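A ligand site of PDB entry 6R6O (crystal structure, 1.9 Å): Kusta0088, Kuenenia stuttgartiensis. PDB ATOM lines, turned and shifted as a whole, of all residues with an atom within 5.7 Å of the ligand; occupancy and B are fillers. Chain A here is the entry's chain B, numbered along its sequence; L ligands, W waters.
Water W3 lies within hydrogen-bond range of O4 of the ligand and NZ of Lys 72.
Water W2 bridges the side-chain hydroxyl of Ser 58 and an oxygen (O2) of the ligand.
An oxygen (O2) of the ligand lies close to the side-chain sulfur (SD) of Met 59 (3.7 Å).
A nitrogen (N1) of the ligand sits close to a ring nitrogen (NE2) of His 67 (3.3 Å).
O of Gln 25 touches C26 of the ligand (3.5 Å).
Glu 26 touches the ligand (C to C24, 3.8 Å).
Ser 27 touches the ligand.
O of Phe 45 touches C31 of the ligand (3.2 Å).
Gly 46 touches the ligand.
Val 47 touches the ligand (CG1 to C27, 3.6 Å).
Pro 48 touches the ligand (CD to C1, 3.8 Å).
Phe 50 touches the ligand (CZ to C8, 3.6 Å).
CE1 of Phe 55 touches C10 of the ligand, at 3.7 Å.
Ile 68 touches the ligand.
O of Lys 72 touches C33 of the ligand, 3.9 Å away.
O of Lys 74 touches C26 of the ligand (3.4 Å).
CD of Pro 76 touches C21 of the ligand (3.6 Å).
OH of Tyr 78 touches C3 of the ligand (3.4 Å).
CE of Met 82 touches C19 of the ligand (3.9 Å).
Met 90 touches the ligand (CG to C17, 3.5 Å).
Val 94 touches the ligand (CG1 to C9, 3.99 Å).
Hydrophobic or aromatic side chains that line the ligand: His 32, Phe 45, Val 47, Pro 48, Phe 50, Phe 55, Met 59, His 67, Ile 68, Pro 76, Tyr 78, Met 82, Met 90 and Val 94.
The nearest printed residue that does not touch the ligand is Ile 64 (4.1 Å).
OH of Tyr 17 is in hydrogen-bond range of O of His 32, at 2.8 Å.
NE2 of His 67 sits close to SG of Cys 75 (3.1 Å).
The backbone carbonyl oxygen (O) of Val 24 sits close to the side-chain hydroxyl (OG) of Ser 27 (3.5 Å).
The backbone carbonyl oxygen (O) of Ile 68 sits at hydrogen-bond distance from the backbone NH (N) of Tyr 78.
The side-chain hydroxyl (OH) of Tyr 78 sits at hydrogen-bond distance from the backbone carbonyl oxygen (O) of Glu 26 (2.7 Å).
N of Val 47 lies within hydrogen-bond range of O of Gly 42 (3.0 Å).
O of Phe 55 is in hydrogen-bond range of OG of Ser 58, 2.6 Å away.
SG of Cys 28 is covalently linked to C18 of the ligand, 1.8 Å away.
The side-chain sulfur (SG) of Cys 31 is covalently linked to a carbon (C25) of the ligand, at 1.8 Å.
NE2 of His 32 binds FE1 of the ligand, 2.2 Å away.
The side-chain sulfur (SG) of Cys 75 binds an iron atom (FE1) of the ligand, 2.5 Å away.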
ATOM      1  N   ILE A  16     -32.446  11.363  -0.368  1.00  0.00           N
ATOM      2  CA  ILE A  16     -31.195  10.773  -0.866  1.00  0.00           C
ATOM      3  C   ILE A  16     -29.987  11.452  -0.213  1.00  0.00           C
ATOM      4  O   ILE A  16     -29.067  10.789   0.257  1.00  0.00           O
ATOM      5  CB  ILE A  16     -31.143  10.880  -2.395  1.00  0.00           C
ATOM      6  CG1 ILE A  16     -32.290  10.095  -3.039  1.00  0.00           C
ATOM      7  CG2 ILE A  16     -29.766  10.400  -2.924  1.00  0.00           C
ATOM      8  CD1 ILE A  16     -32.339   8.660  -2.634  1.00  0.00           C
ATOM      9  N   TYR A  17     -29.998  12.783  -0.162  1.00  0.00           N
ATOM     10  CA  TYR A  17     -28.927  13.541   0.484  1.00  0.00           C
ATOM     11  C   TYR A  17     -28.767  13.110   1.935  1.00  0.00           C
ATOM     12  O   TYR A  17     -27.648  13.086   2.466  1.00  0.00           O
ATOM     13  CB  TYR A  17     -29.266  15.031   0.398  1.00  0.00           C
ATOM     14  CG  TYR A  17     -28.162  16.047   0.705  1.00  0.00           C
ATOM     15  CD1 TYR A  17     -27.756  16.327   2.008  1.00  0.00           C
ATOM     16  CD2 TYR A  17     -27.569  16.758  -0.333  1.00  0.00           C
ATOM     17  CE1 TYR A  17     -26.769  17.306   2.243  1.00  0.00           C
ATOM     18  CE2 TYR A  17     -26.614  17.705  -0.103  1.00  0.00           C
ATOM     19  CZ  TYR A  17     -26.212  17.985   1.180  1.00  0.00           C
ATOM     20  OH  TYR A  17     -25.241  18.952   1.357  1.00  0.00           O
ATOM     21  N   VAL A  24     -23.665   5.392   5.603  1.00  0.00           N
ATOM     22  CA  VAL A  24     -23.499   6.731   6.151  1.00  0.00           C
ATOM     23  C   VAL A  24     -22.315   7.444   5.500  1.00  0.00           C
ATOM     24  O   VAL A  24     -22.427   8.601   5.080  1.00  0.00           O
ATOM     25  CB  VAL A  24     -23.339   6.666   7.685  1.00  0.00           C
ATOM     26  CG1 VAL A  24     -22.879   8.015   8.214  1.00  0.00           C
ATOM     27  CG2 VAL A  24     -24.641   6.274   8.328  1.00  0.00           C
ATOM     28  N   GLN A  25     -21.181   6.756   5.386  1.00  0.00           N
ATOM     29  CA  GLN A  25     -20.001   7.399   4.817  1.00  0.00           C
ATOM     30  C   GLN A  25     -20.128   7.664   3.329  1.00  0.00           C
ATOM     31  O   GLN A  25     -19.257   8.325   2.760  1.00  0.00           O
ATOM     32  CB  GLN A  25     -18.750   6.536   5.088  1.00  0.00           C
ATOM     33  CG  GLN A  25     -18.457   6.309   6.558  1.00  0.00           C
ATOM     34  CD  GLN A  25     -17.430   5.211   6.784  1.00  0.00           C
ATOM     35  OE1 GLN A  25     -17.704   4.038   6.529  1.00  0.00           O
ATOM     36  NE2 GLN A  25     -16.256   5.581   7.269  1.00  0.00           N
ATOM     37  N   GLU A  26     -21.188   7.196   2.672  1.00  0.00           N
ATOM     38  CA  GLU A  26     -21.423   7.534   1.274  1.00  0.00           C
ATOM     39  C   GLU A  26     -22.657   8.419   1.091  1.00  0.00           C
ATOM     40  O   GLU A  26     -23.194   8.504  -0.014  1.00  0.00           O
ATOM     41  CB  GLU A  26     -21.553   6.258   0.436  1.00  0.00           C
ATOM     42  CG  GLU A  26     -20.780   6.286  -0.880  1.00  0.00           C
ATOM     43  CD  GLU A  26     -21.178   5.168  -1.824  1.00  0.00           C
ATOM     44  OE1 GLU A  26     -21.542   4.083  -1.323  1.00  0.00           O
ATOM     45  OE2 GLU A  26     -21.142   5.367  -3.056  1.00  0.00           O
ATOM     46  N   SER A  27     -23.105   9.074   2.154  1.00  0.00           N
ATOM     47  CA  SER A  27     -24.290   9.933   2.136  1.00  0.00           C
ATOM     48  C   SER A  27     -23.841  11.384   2.171  1.00  0.00           C
ATOM     49  O   SER A  27     -22.992  11.734   2.993  1.00  0.00           O
ATOM     50  CB  SER A  27     -25.204   9.641   3.322  1.00  0.00           C
ATOM     51  OG  SER A  27     -25.453   8.249   3.457  1.00  0.00           O
ATOM     52  N   CYS A  28     -24.421  12.225   1.290  1.00  0.00           N
ATOM     53  CA  CYS A  28     -23.984  13.626   1.205  1.00  0.00           C
ATOM     54  C   CYS A  28     -23.931  14.288   2.579  1.00  0.00           C
ATOM     55  O   CYS A  28     -22.978  14.984   2.900  1.00  0.00           O
ATOM     56  CB  CYS A  28     -24.908  14.445   0.280  1.00  0.00           C
ATOM     57  SG  CYS A  28     -25.499  13.724  -1.288  1.00  0.00           S
ATOM     58  N   TYR A  30     -23.358  13.332   5.509  1.00  0.00           N
ATOM     59  CA  TYR A  30     -22.279  12.972   6.420  1.00  0.00           C
ATOM     60  C   TYR A  30     -21.081  13.892   6.245  1.00  0.00           C
ATOM     61  O   TYR A  30     -20.363  14.166   7.211  1.00  0.00           O
ATOM     62  CB  TYR A  30     -21.885  11.520   6.213  1.00  0.00           C
ATOM     63  CG  TYR A  30     -20.732  11.051   7.081  1.00  0.00           C
ATOM     64  CD1 TYR A  30     -20.902  10.838   8.447  1.00  0.00           C
ATOM     65  CD2 TYR A  30     -19.484  10.803   6.535  1.00  0.00           C
ATOM     66  CE1 TYR A  30     -19.856  10.399   9.252  1.00  0.00           C
ATOM     67  CE2 TYR A  30     -18.430  10.367   7.329  1.00  0.00           C
ATOM     68  CZ  TYR A  30     -18.620  10.170   8.678  1.00  0.00           C
ATOM     69  OH  TYR A  30     -17.566   9.725   9.451  1.00  0.00           O
ATOM     70  N   CYS A  31     -20.856  14.380   5.034  1.00  0.00           N
ATOM     71  CA  CYS A  31     -19.766  15.303   4.724  1.00  0.00           C
ATOM     72  C   CYS A  31     -20.236  16.716   4.457  1.00  0.00           C
ATOM     73  O   CYS A  31     -19.533  17.672   4.811  1.00  0.00           O
ATOM     74  CB  CYS A  31     -18.995  14.805   3.486  1.00  0.00           C
ATOM     75  SG  CYS A  31     -18.265  13.119   3.627  1.00  0.00           S
ATOM     76  N   HIS A  32     -21.401  16.879   3.823  1.00  0.00           N
ATOM     77  CA  HIS A  32     -21.915  18.188   3.451  1.00  0.00           C
ATOM     78  C   HIS A  32     -23.106  18.596   4.302  1.00  0.00           C
ATOM     79  O   HIS A  32     -23.947  19.371   3.840  1.00  0.00           O
ATOM     80  CB  HIS A  32     -22.313  18.229   1.986  1.00  0.00           C
ATOM     81  CG  HIS A  32     -21.185  18.008   1.035  1.00  0.00           C
ATOM     82  ND1 HIS A  32     -20.145  18.903   0.886  1.00  0.00           N
ATOM     83  CD2 HIS A  32     -20.934  17.005   0.165  1.00  0.00           C
ATOM     84  CE1 HIS A  32     -19.308  18.460  -0.028  1.00  0.00           C
ATOM     85  NE2 HIS A  32     -19.759  17.301  -0.477  1.00  0.00           N
ATOM     86  N   GLY A  42     -16.600  16.142   7.280  1.00  0.00           N
ATOM     87  CA  GLY A  42     -16.475  16.729   5.944  1.00  0.00           C
ATOM     88  C   GLY A  42     -15.335  17.730   5.850  1.00  0.00           C
ATOM     89  O   GLY A  42     -14.604  17.754   4.855  1.00  0.00           O
ATOM     90  N   PHE A  45     -12.032  16.129   5.528  1.00  0.00           N
ATOM     91  CA  PHE A  45     -11.825  15.621   4.172  1.00  0.00           C
ATOM     92  C   PHE A  45     -11.634  16.732   3.143  1.00  0.00           C
ATOM     93  O   PHE A  45     -11.230  16.438   2.018  1.00  0.00           O
ATOM     94  CB  PHE A  45     -13.012  14.744   3.737  1.00  0.00           C
ATOM     95  CG  PHE A  45     -13.213  13.514   4.575  1.00  0.00           C
ATOM     96  CD1 PHE A  45     -12.136  12.916   5.222  1.00  0.00           C
ATOM     97  CD2 PHE A  45     -14.474  12.957   4.713  1.00  0.00           C
ATOM     98  CE1 PHE A  45     -12.318  11.782   5.996  1.00  0.00           C
ATOM     99  CE2 PHE A  45     -14.662  11.810   5.487  1.00  0.00           C
ATOM    100  CZ  PHE A  45     -13.593  11.231   6.126  1.00  0.00           C
ATOM    101  N   GLY A  46     -11.918  17.979   3.502  1.00  0.00           N
ATOM    102  CA  GLY A  46     -11.727  19.092   2.605  1.00  0.00           C
ATOM    103  C   GLY A  46     -12.941  19.597   1.839  1.00  0.00           C
ATOM    104  O   GLY A  46     -12.772  20.142   0.739  1.00  0.00           O
ATOM    105  N   VAL A  47     -14.153  19.444   2.376  1.00  0.00           N
ATOM    106  CA  VAL A  47     -15.354  19.867   1.638  1.00  0.00           C
ATOM    107  C   VAL A  47     -15.348  21.378   1.464  1.00  0.00           C
ATOM    108  O   VAL A  47     -14.879  22.100   2.363  1.00  0.00           O
ATOM    109  CB  VAL A  47     -16.681  19.442   2.315  1.00  0.00           C
ATOM    110  CG1 VAL A  47     -16.829  17.920   2.381  1.00  0.00           C
ATOM    111  CG2 VAL A  47     -16.819  20.068   3.690  1.00  0.00           C
ATOM    112  N   PRO A  48     -15.878  21.890   0.359  1.00  0.00           N
ATOM    113  CA  PRO A  48     -16.136  23.325   0.249  1.00  0.00           C
ATOM    114  C   PRO A  48     -17.407  23.701   1.003  1.00  0.00           C
ATOM    115  O   PRO A  48     -18.138  22.859   1.506  1.00  0.00           O
ATOM    116  CB  PRO A  48     -16.317  23.519  -1.261  1.00  0.00           C
ATOM    117  CG  PRO A  48     -16.915  22.202  -1.706  1.00  0.00           C
ATOM    118  CD  PRO A  48     -16.227  21.158  -0.874  1.00  0.00           C
ATOM    119  N   PHE A  50     -20.959  25.053   0.706  1.00  0.00           N
ATOM    120  CA  PHE A  50     -22.033  25.259  -0.258  1.00  0.00           C
ATOM    121  C   PHE A  50     -22.806  26.554  -0.019  1.00  0.00           C
ATOM    122  O   PHE A  50     -23.519  27.010  -0.921  1.00  0.00           O
ATOM    123  CB  PHE A  50     -23.048  24.093  -0.227  1.00  0.00           C
ATOM    124  CG  PHE A  50     -22.537  22.780  -0.787  1.00  0.00           C
ATOM    125  CD1 PHE A  50     -21.377  22.706  -1.551  1.00  0.00           C
ATOM    126  CD2 PHE A  50     -23.253  21.600  -0.542  1.00  0.00           C
ATOM    127  CE1 PHE A  50     -20.930  21.474  -2.059  1.00  0.00           C
ATOM    128  CE2 PHE A  50     -22.832  20.380  -1.057  1.00  0.00           C
ATOM    129  CZ  PHE A  50     -21.662  20.309  -1.812  1.00  0.00           C
ATOM    130  N   PHE A  55     -17.682  29.735  -3.457  1.00  0.00           N
ATOM    131  CA  PHE A  55     -17.774  28.365  -3.947  1.00  0.00           C
ATOM    132  C   PHE A  55     -18.716  28.281  -5.138  1.00  0.00           C
ATOM    133  O   PHE A  55     -18.371  27.716  -6.173  1.00  0.00           O
ATOM    134  CB  PHE A  55     -18.267  27.390  -2.886  1.00  0.00           C
ATOM    135  CG  PHE A  55     -18.782  26.101  -3.477  1.00  0.00           C
ATOM    136  CD1 PHE A  55     -17.888  25.162  -3.968  1.00  0.00           C
ATOM    137  CD2 PHE A  55     -20.145  25.876  -3.624  1.00  0.00           C
ATOM    138  CE1 PHE A  55     -18.331  24.013  -4.539  1.00  0.00           C
ATOM    139  CE2 PHE A  55     -20.596  24.715  -4.205  1.00  0.00           C
ATOM    140  CZ  PHE A  55     -19.696  23.775  -4.656  1.00  0.00           C
ATOM    141  N   SER A  58     -17.565  29.171  -8.520  1.00  0.00           N
ATOM    142  CA  SER A  58     -16.483  28.376  -9.052  1.00  0.00           C
ATOM    143  C   SER A  58     -16.952  27.217  -9.933  1.00  0.00           C
ATOM    144  O   SER A  58     -16.115  26.553 -10.554  1.00  0.00           O
ATOM    145  CB  SER A  58     -15.600  27.826  -7.915  1.00  0.00           C
ATOM    146  OG  SER A  58     -16.207  26.710  -7.263  1.00  0.00           O
ATOM    147  N   MET A  59     -18.267  26.973 -10.018  1.00  0.00           N
ATOM    148  CA  MET A  59     -18.824  25.872 -10.783  1.00  0.00           C
ATOM    149  C   MET A  59     -20.023  26.343 -11.602  1.00  0.00           C
ATOM    150  O   MET A  59     -20.815  27.161 -11.150  1.00  0.00           O
ATOM    151  CB  MET A  59     -19.245  24.719  -9.867  1.00  0.00           C
ATOM    152  CG  MET A  59     -18.113  24.149  -9.027  1.00  0.00           C
ATOM    153  SD  MET A  59     -18.595  22.647  -8.133  1.00  0.00           S
ATOM    154  CE  MET A  59     -18.549  21.434  -9.467  1.00  0.00           C
ATOM    155  N   ILE A  64     -21.495  20.908 -11.895  1.00  0.00           N
ATOM    156  CA  ILE A  64     -22.022  20.231 -10.706  1.00  0.00           C
ATOM    157  C   ILE A  64     -22.619  18.879 -11.090  1.00  0.00           C
ATOM    158  O   ILE A  64     -22.356  17.856 -10.441  1.00  0.00           O
ATOM    159  CB  ILE A  64     -23.042  21.121  -9.981  1.00  0.00           C
ATOM    160  CG1 ILE A  64     -22.372  22.369  -9.386  1.00  0.00           C
ATOM    161  CG2 ILE A  64     -23.703  20.348  -8.840  1.00  0.00           C
ATOM    162  CD1 ILE A  64     -23.365  23.314  -8.706  1.00  0.00           C
ATOM    163  N   HIS A  67     -19.835  16.572 -11.866  1.00  0.00           N
ATOM    164  CA  HIS A  67     -19.102  16.199 -10.664  1.00  0.00           C
ATOM    165  C   HIS A  67     -19.826  15.099  -9.900  1.00  0.00           C
ATOM    166  O   HIS A  67     -19.207  14.102  -9.513  1.00  0.00           O
ATOM    167  CB  HIS A  67     -18.877  17.397  -9.741  1.00  0.00           C
ATOM    168  CG  HIS A  67     -18.382  16.982  -8.376  1.00  0.00           C
ATOM    169  ND1 HIS A  67     -17.055  16.741  -8.104  1.00  0.00           N
ATOM    170  CD2 HIS A  67     -19.061  16.702  -7.240  1.00  0.00           C
ATOM    171  CE1 HIS A  67     -16.924  16.364  -6.841  1.00  0.00           C
ATOM    172  NE2 HIS A  67     -18.134  16.329  -6.293  1.00  0.00           N
ATOM    173  N   ILE A  68     -21.125  15.273  -9.629  1.00  0.00           N
ATOM    174  CA  ILE A  68     -21.861  14.264  -8.873  1.00  0.00           C
ATOM    175  C   ILE A  68     -21.780  12.915  -9.574  1.00  0.00           C
ATOM    176  O   ILE A  68     -21.663  11.874  -8.931  1.00  0.00           O
ATOM    177  CB  ILE A  68     -23.327  14.701  -8.644  1.00  0.00           C
ATOM    178  CG1 ILE A  68     -23.386  15.950  -7.765  1.00  0.00           C
ATOM    179  CG2 ILE A  68     -24.126  13.550  -7.990  1.00  0.00           C
ATOM    180  CD1 ILE A  68     -24.716  16.722  -7.871  1.00  0.00           C
ATOM    181  N   LYS A  72     -14.875  13.047  -6.982  1.00  0.00           N
ATOM    182  CA  LYS A  72     -13.526  13.587  -7.013  1.00  0.00           C
ATOM    183  C   LYS A  72     -12.930  13.377  -5.634  1.00  0.00           C
ATOM    184  O   LYS A  72     -13.482  13.840  -4.636  1.00  0.00           O
ATOM    185  CB  LYS A  72     -13.495  15.087  -7.384  1.00  0.00           C
ATOM    186  CG  LYS A  72     -12.072  15.639  -7.529  1.00  0.00           C
ATOM    187  CD  LYS A  72     -12.031  17.086  -8.014  1.00  0.00           C
ATOM    188  CE  LYS A  72     -10.581  17.535  -8.224  1.00  0.00           C
ATOM    189  NZ  LYS A  72     -10.470  18.943  -8.701  1.00  0.00           N
ATOM    190  N   GLY A  73     -11.820  12.658  -5.572  1.00  0.00           N
ATOM    191  CA  GLY A  73     -11.174  12.441  -4.292  1.00  0.00           C
ATOM    192  C   GLY A  73     -12.079  11.639  -3.385  1.00  0.00           C
ATOM    193  O   GLY A  73     -12.578  10.563  -3.744  1.00  0.00           O
ATOM    194  N   LYS A  74     -12.305  12.183  -2.198  1.00  0.00           N
ATOM    195  CA  LYS A  74     -13.184  11.546  -1.232  1.00  0.00           C
ATOM    196  C   LYS A  74     -14.662  11.779  -1.520  1.00  0.00           C
ATOM    197  O   LYS A  74     -15.499  11.145  -0.876  1.00  0.00           O
ATOM    198  CB  LYS A  74     -12.856  12.058   0.176  1.00  0.00           C
ATOM    199  CG  LYS A  74     -11.433  11.757   0.574  1.00  0.00           C
ATOM    200  CD  LYS A  74     -11.270  11.790   2.078  1.00  0.00           C
ATOM    201  CE  LYS A  74      -9.827  11.499   2.422  1.00  0.00           C
ATOM    202  NZ  LYS A  74      -9.374  10.329   1.628  1.00  0.00           N
ATOM    203  N   CYS A  75     -14.996  12.666  -2.442  1.00  0.00           N
ATOM    204  CA  CYS A  75     -16.384  12.792  -2.877  1.00  0.00           C
ATOM    205  C   CYS A  75     -16.701  11.636  -3.804  1.00  0.00           C
ATOM    206  O   CYS A  75     -16.085  11.529  -4.872  1.00  0.00           O
ATOM    207  CB  CYS A  75     -16.617  14.116  -3.600  1.00  0.00           C
ATOM    208  SG  CYS A  75     -18.383  14.456  -3.839  1.00  0.00           S
ATOM    209  N   PRO A  76     -17.620  10.748  -3.432  1.00  0.00           N
ATOM    210  CA  PRO A  76     -17.851   9.539  -4.222  1.00  0.00           C
ATOM    211  C   PRO A  76     -18.467   9.847  -5.577  1.00  0.00           C
ATOM    212  O   PRO A  76     -19.102  10.880  -5.788  1.00  0.00           O
ATOM    213  CB  PRO A  76     -18.836   8.733  -3.352  1.00  0.00           C
ATOM    214  CG  PRO A  76     -18.694   9.299  -1.973  1.00  0.00           C
ATOM    215  CD  PRO A  76     -18.397  10.765  -2.176  1.00  0.00           C
ATOM    216  N   TYR A  78     -21.448   9.058  -8.072  1.00  0.00           N
ATOM    217  CA  TYR A  78     -22.825   8.618  -7.924  1.00  0.00           C
ATOM    218  C   TYR A  78     -23.505   8.231  -9.232  1.00  0.00           C
ATOM    219  O   TYR A  78     -24.688   7.879  -9.218  1.00  0.00           O
ATOM    220  CB  TYR A  78     -23.668   9.699  -7.208  1.00  0.00           C
ATOM    221  CG  TYR A  78     -23.259   9.854  -5.765  1.00  0.00           C
ATOM    222  CD1 TYR A  78     -23.852   9.071  -4.758  1.00  0.00           C
ATOM    223  CD2 TYR A  78     -22.245  10.728  -5.403  1.00  0.00           C
ATOM    224  CE1 TYR A  78     -23.464   9.205  -3.423  1.00  0.00           C
ATOM    225  CE2 TYR A  78     -21.842  10.856  -4.060  1.00  0.00           C
ATOM    226  CZ  TYR A  78     -22.452  10.101  -3.090  1.00  0.00           C
ATOM    227  OH  TYR A  78     -22.054  10.252  -1.787  1.00  0.00           O
ATOM    228  N   MET A  82     -27.970   6.827  -8.652  1.00  0.00           N
ATOM    229  CA  MET A  82     -29.250   7.517  -8.697  1.00  0.00           C
ATOM    230  C   MET A  82     -29.482   7.912 -10.146  1.00  0.00           C
ATOM    231  O   MET A  82     -28.538   7.936 -10.953  1.00  0.00           O
ATOM    232  CB  MET A  82     -29.291   8.725  -7.739  1.00  0.00           C
ATOM    233  CG  MET A  82     -28.312   9.832  -8.049  1.00  0.00           C
ATOM    234  SD  MET A  82     -28.349  11.241  -6.888  1.00  0.00           S
ATOM    235  CE  MET A  82     -27.296  10.623  -5.589  1.00  0.00           C
ATOM    236  N   MET A  90     -30.346  16.916  -7.451  1.00  0.00           N
ATOM    237  CA  MET A  90     -29.299  17.069  -6.449  1.00  0.00           C
ATOM    238  C   MET A  90     -28.432  18.294  -6.729  1.00  0.00           C
ATOM    239  O   MET A  90     -28.003  18.990  -5.804  1.00  0.00           O
ATOM    240  CB  MET A  90     -28.443  15.805  -6.388  1.00  0.00           C
ATOM    241  CG  MET A  90     -27.732  15.639  -5.059  1.00  0.00           C
ATOM    242  SD  MET A  90     -28.906  15.403  -3.696  1.00  0.00           S
ATOM    243  CE  MET A  90     -29.826  14.015  -4.291  1.00  0.00           C
ATOM    244  N   VAL A  94     -27.559  21.451  -4.180  1.00  0.00           N
ATOM    245  CA  VAL A  94     -26.263  22.091  -3.927  1.00  0.00           C
ATOM    246  C   VAL A  94     -26.378  23.602  -4.112  1.00  0.00           C
ATOM    247  O   VAL A  94     -25.897  24.385  -3.265  1.00  0.00           O
ATOM    248  CB  VAL A  94     -25.179  21.501  -4.843  1.00  0.00           C
ATOM    249  CG1 VAL A  94     -23.862  22.352  -4.776  1.00  0.00           C
ATOM    250  CG2 VAL A  94     -24.909  20.064  -4.471  1.00  0.00           C
HETATM  251 FE1  LIG L   1     -19.120  15.927  -2.022  1.00  0.00          FE
HETATM  252  C1  LIG L   1     -16.887  18.311  -3.276  1.00  0.00           C
HETATM  253  C2  LIG L   1     -21.579  17.241  -3.984  1.00  0.00           C
HETATM  254  C3  LIG L   1     -21.252  13.451  -0.939  1.00  0.00           C
HETATM  255  C4  LIG L   1     -16.857  14.985   0.350  1.00  0.00           C
HETATM  256  N1  LIG L   1     -19.206  17.481  -3.367  1.00  0.00           N
HETATM  257  C5  LIG L   1     -18.193  18.350  -3.735  1.00  0.00           C
HETATM  258  C6  LIG L   1     -18.746  19.300  -4.671  1.00  0.00           C
HETATM  259  C7  LIG L   1     -20.037  18.997  -4.871  1.00  0.00           C
HETATM  260  C8  LIG L   1     -20.347  17.848  -4.056  1.00  0.00           C
HETATM  261  C9  LIG L   1     -21.037  19.727  -5.804  1.00  0.00           C
HETATM  262  C10 LIG L   1     -17.949  20.451  -5.335  1.00  0.00           C
HETATM  263  C11 LIG L   1     -17.113  19.808  -6.433  1.00  0.00           C
HETATM  264  C12 LIG L   1     -15.729  20.359  -6.297  1.00  0.00           C
HETATM  265  O1  LIG L   1     -14.807  19.521  -6.072  1.00  0.00           O
HETATM  266  O2  LIG L   1     -15.567  21.600  -6.377  1.00  0.00           O
HETATM  267  N2  LIG L   1     -21.045  15.424  -2.392  1.00  0.00           N
HETATM  268  C13 LIG L   1     -21.876  16.093  -3.282  1.00  0.00           C
HETATM  269  C14 LIG L   1     -23.110  15.348  -3.394  1.00  0.00           C
HETATM  270  C15 LIG L   1     -23.045  14.316  -2.529  1.00  0.00           C
HETATM  271  C16 LIG L   1     -21.730  14.333  -1.898  1.00  0.00           C
HETATM  272  C17 LIG L   1     -24.293  15.839  -4.266  1.00  0.00           C
HETATM  273  C18 LIG L   1     -24.100  13.227  -2.246  1.00  0.00           C
HETATM  274  C19 LIG L   1     -24.741  12.628  -3.521  1.00  0.00           C
HETATM  275  N3  LIG L   1     -19.077  14.474  -0.518  1.00  0.00           N
HETATM  276  C20 LIG L   1     -20.047  13.523  -0.269  1.00  0.00           C
HETATM  277  C21 LIG L   1     -19.522  12.590   0.732  1.00  0.00           C
HETATM  278  C22 LIG L   1     -18.311  13.044   1.109  1.00  0.00           C
HETATM  279  C23 LIG L   1     -18.008  14.222   0.315  1.00  0.00           C
HETATM  280  C24 LIG L   1     -20.322  11.380   1.315  1.00  0.00           C
HETATM  281  C25 LIG L   1     -17.400  12.464   2.220  1.00  0.00           C
HETATM  282  C26 LIG L   1     -17.062  10.966   2.093  1.00  0.00           C
HETATM  283  N4  LIG L   1     -17.226  16.570  -1.526  1.00  0.00           N
HETATM  284  C27 LIG L   1     -16.446  15.931  -0.555  1.00  0.00           C
HETATM  285  C28 LIG L   1     -15.093  16.452  -0.607  1.00  0.00           C
HETATM  286  C29 LIG L   1     -15.109  17.475  -1.714  1.00  0.00           C
HETATM  287  C30 LIG L   1     -16.450  17.485  -2.249  1.00  0.00           C
HETATM  288  C31 LIG L   1     -13.885  16.076   0.272  1.00  0.00           C
HETATM  289  C32 LIG L   1     -13.907  18.300  -2.205  1.00  0.00           C
HETATM  290  C33 LIG L   1     -13.445  17.502  -3.433  1.00  0.00           C
HETATM  291  C34 LIG L   1     -12.331  18.245  -4.113  1.00  0.00           C
HETATM  292  O3  LIG L   1     -11.197  17.740  -4.094  1.00  0.00           O
HETATM  293  O4  LIG L   1     -12.553  19.350  -4.667  1.00  0.00           O
HETATM  294  O   HOH W   1     -15.104   8.897   0.230  1.00  0.00           O
HETATM  295  O   HOH W   2     -14.631  24.327  -6.853  1.00  0.00           O
HETATM  296  O   HOH W   3     -11.534  21.000  -6.735  1.00  0.00           O
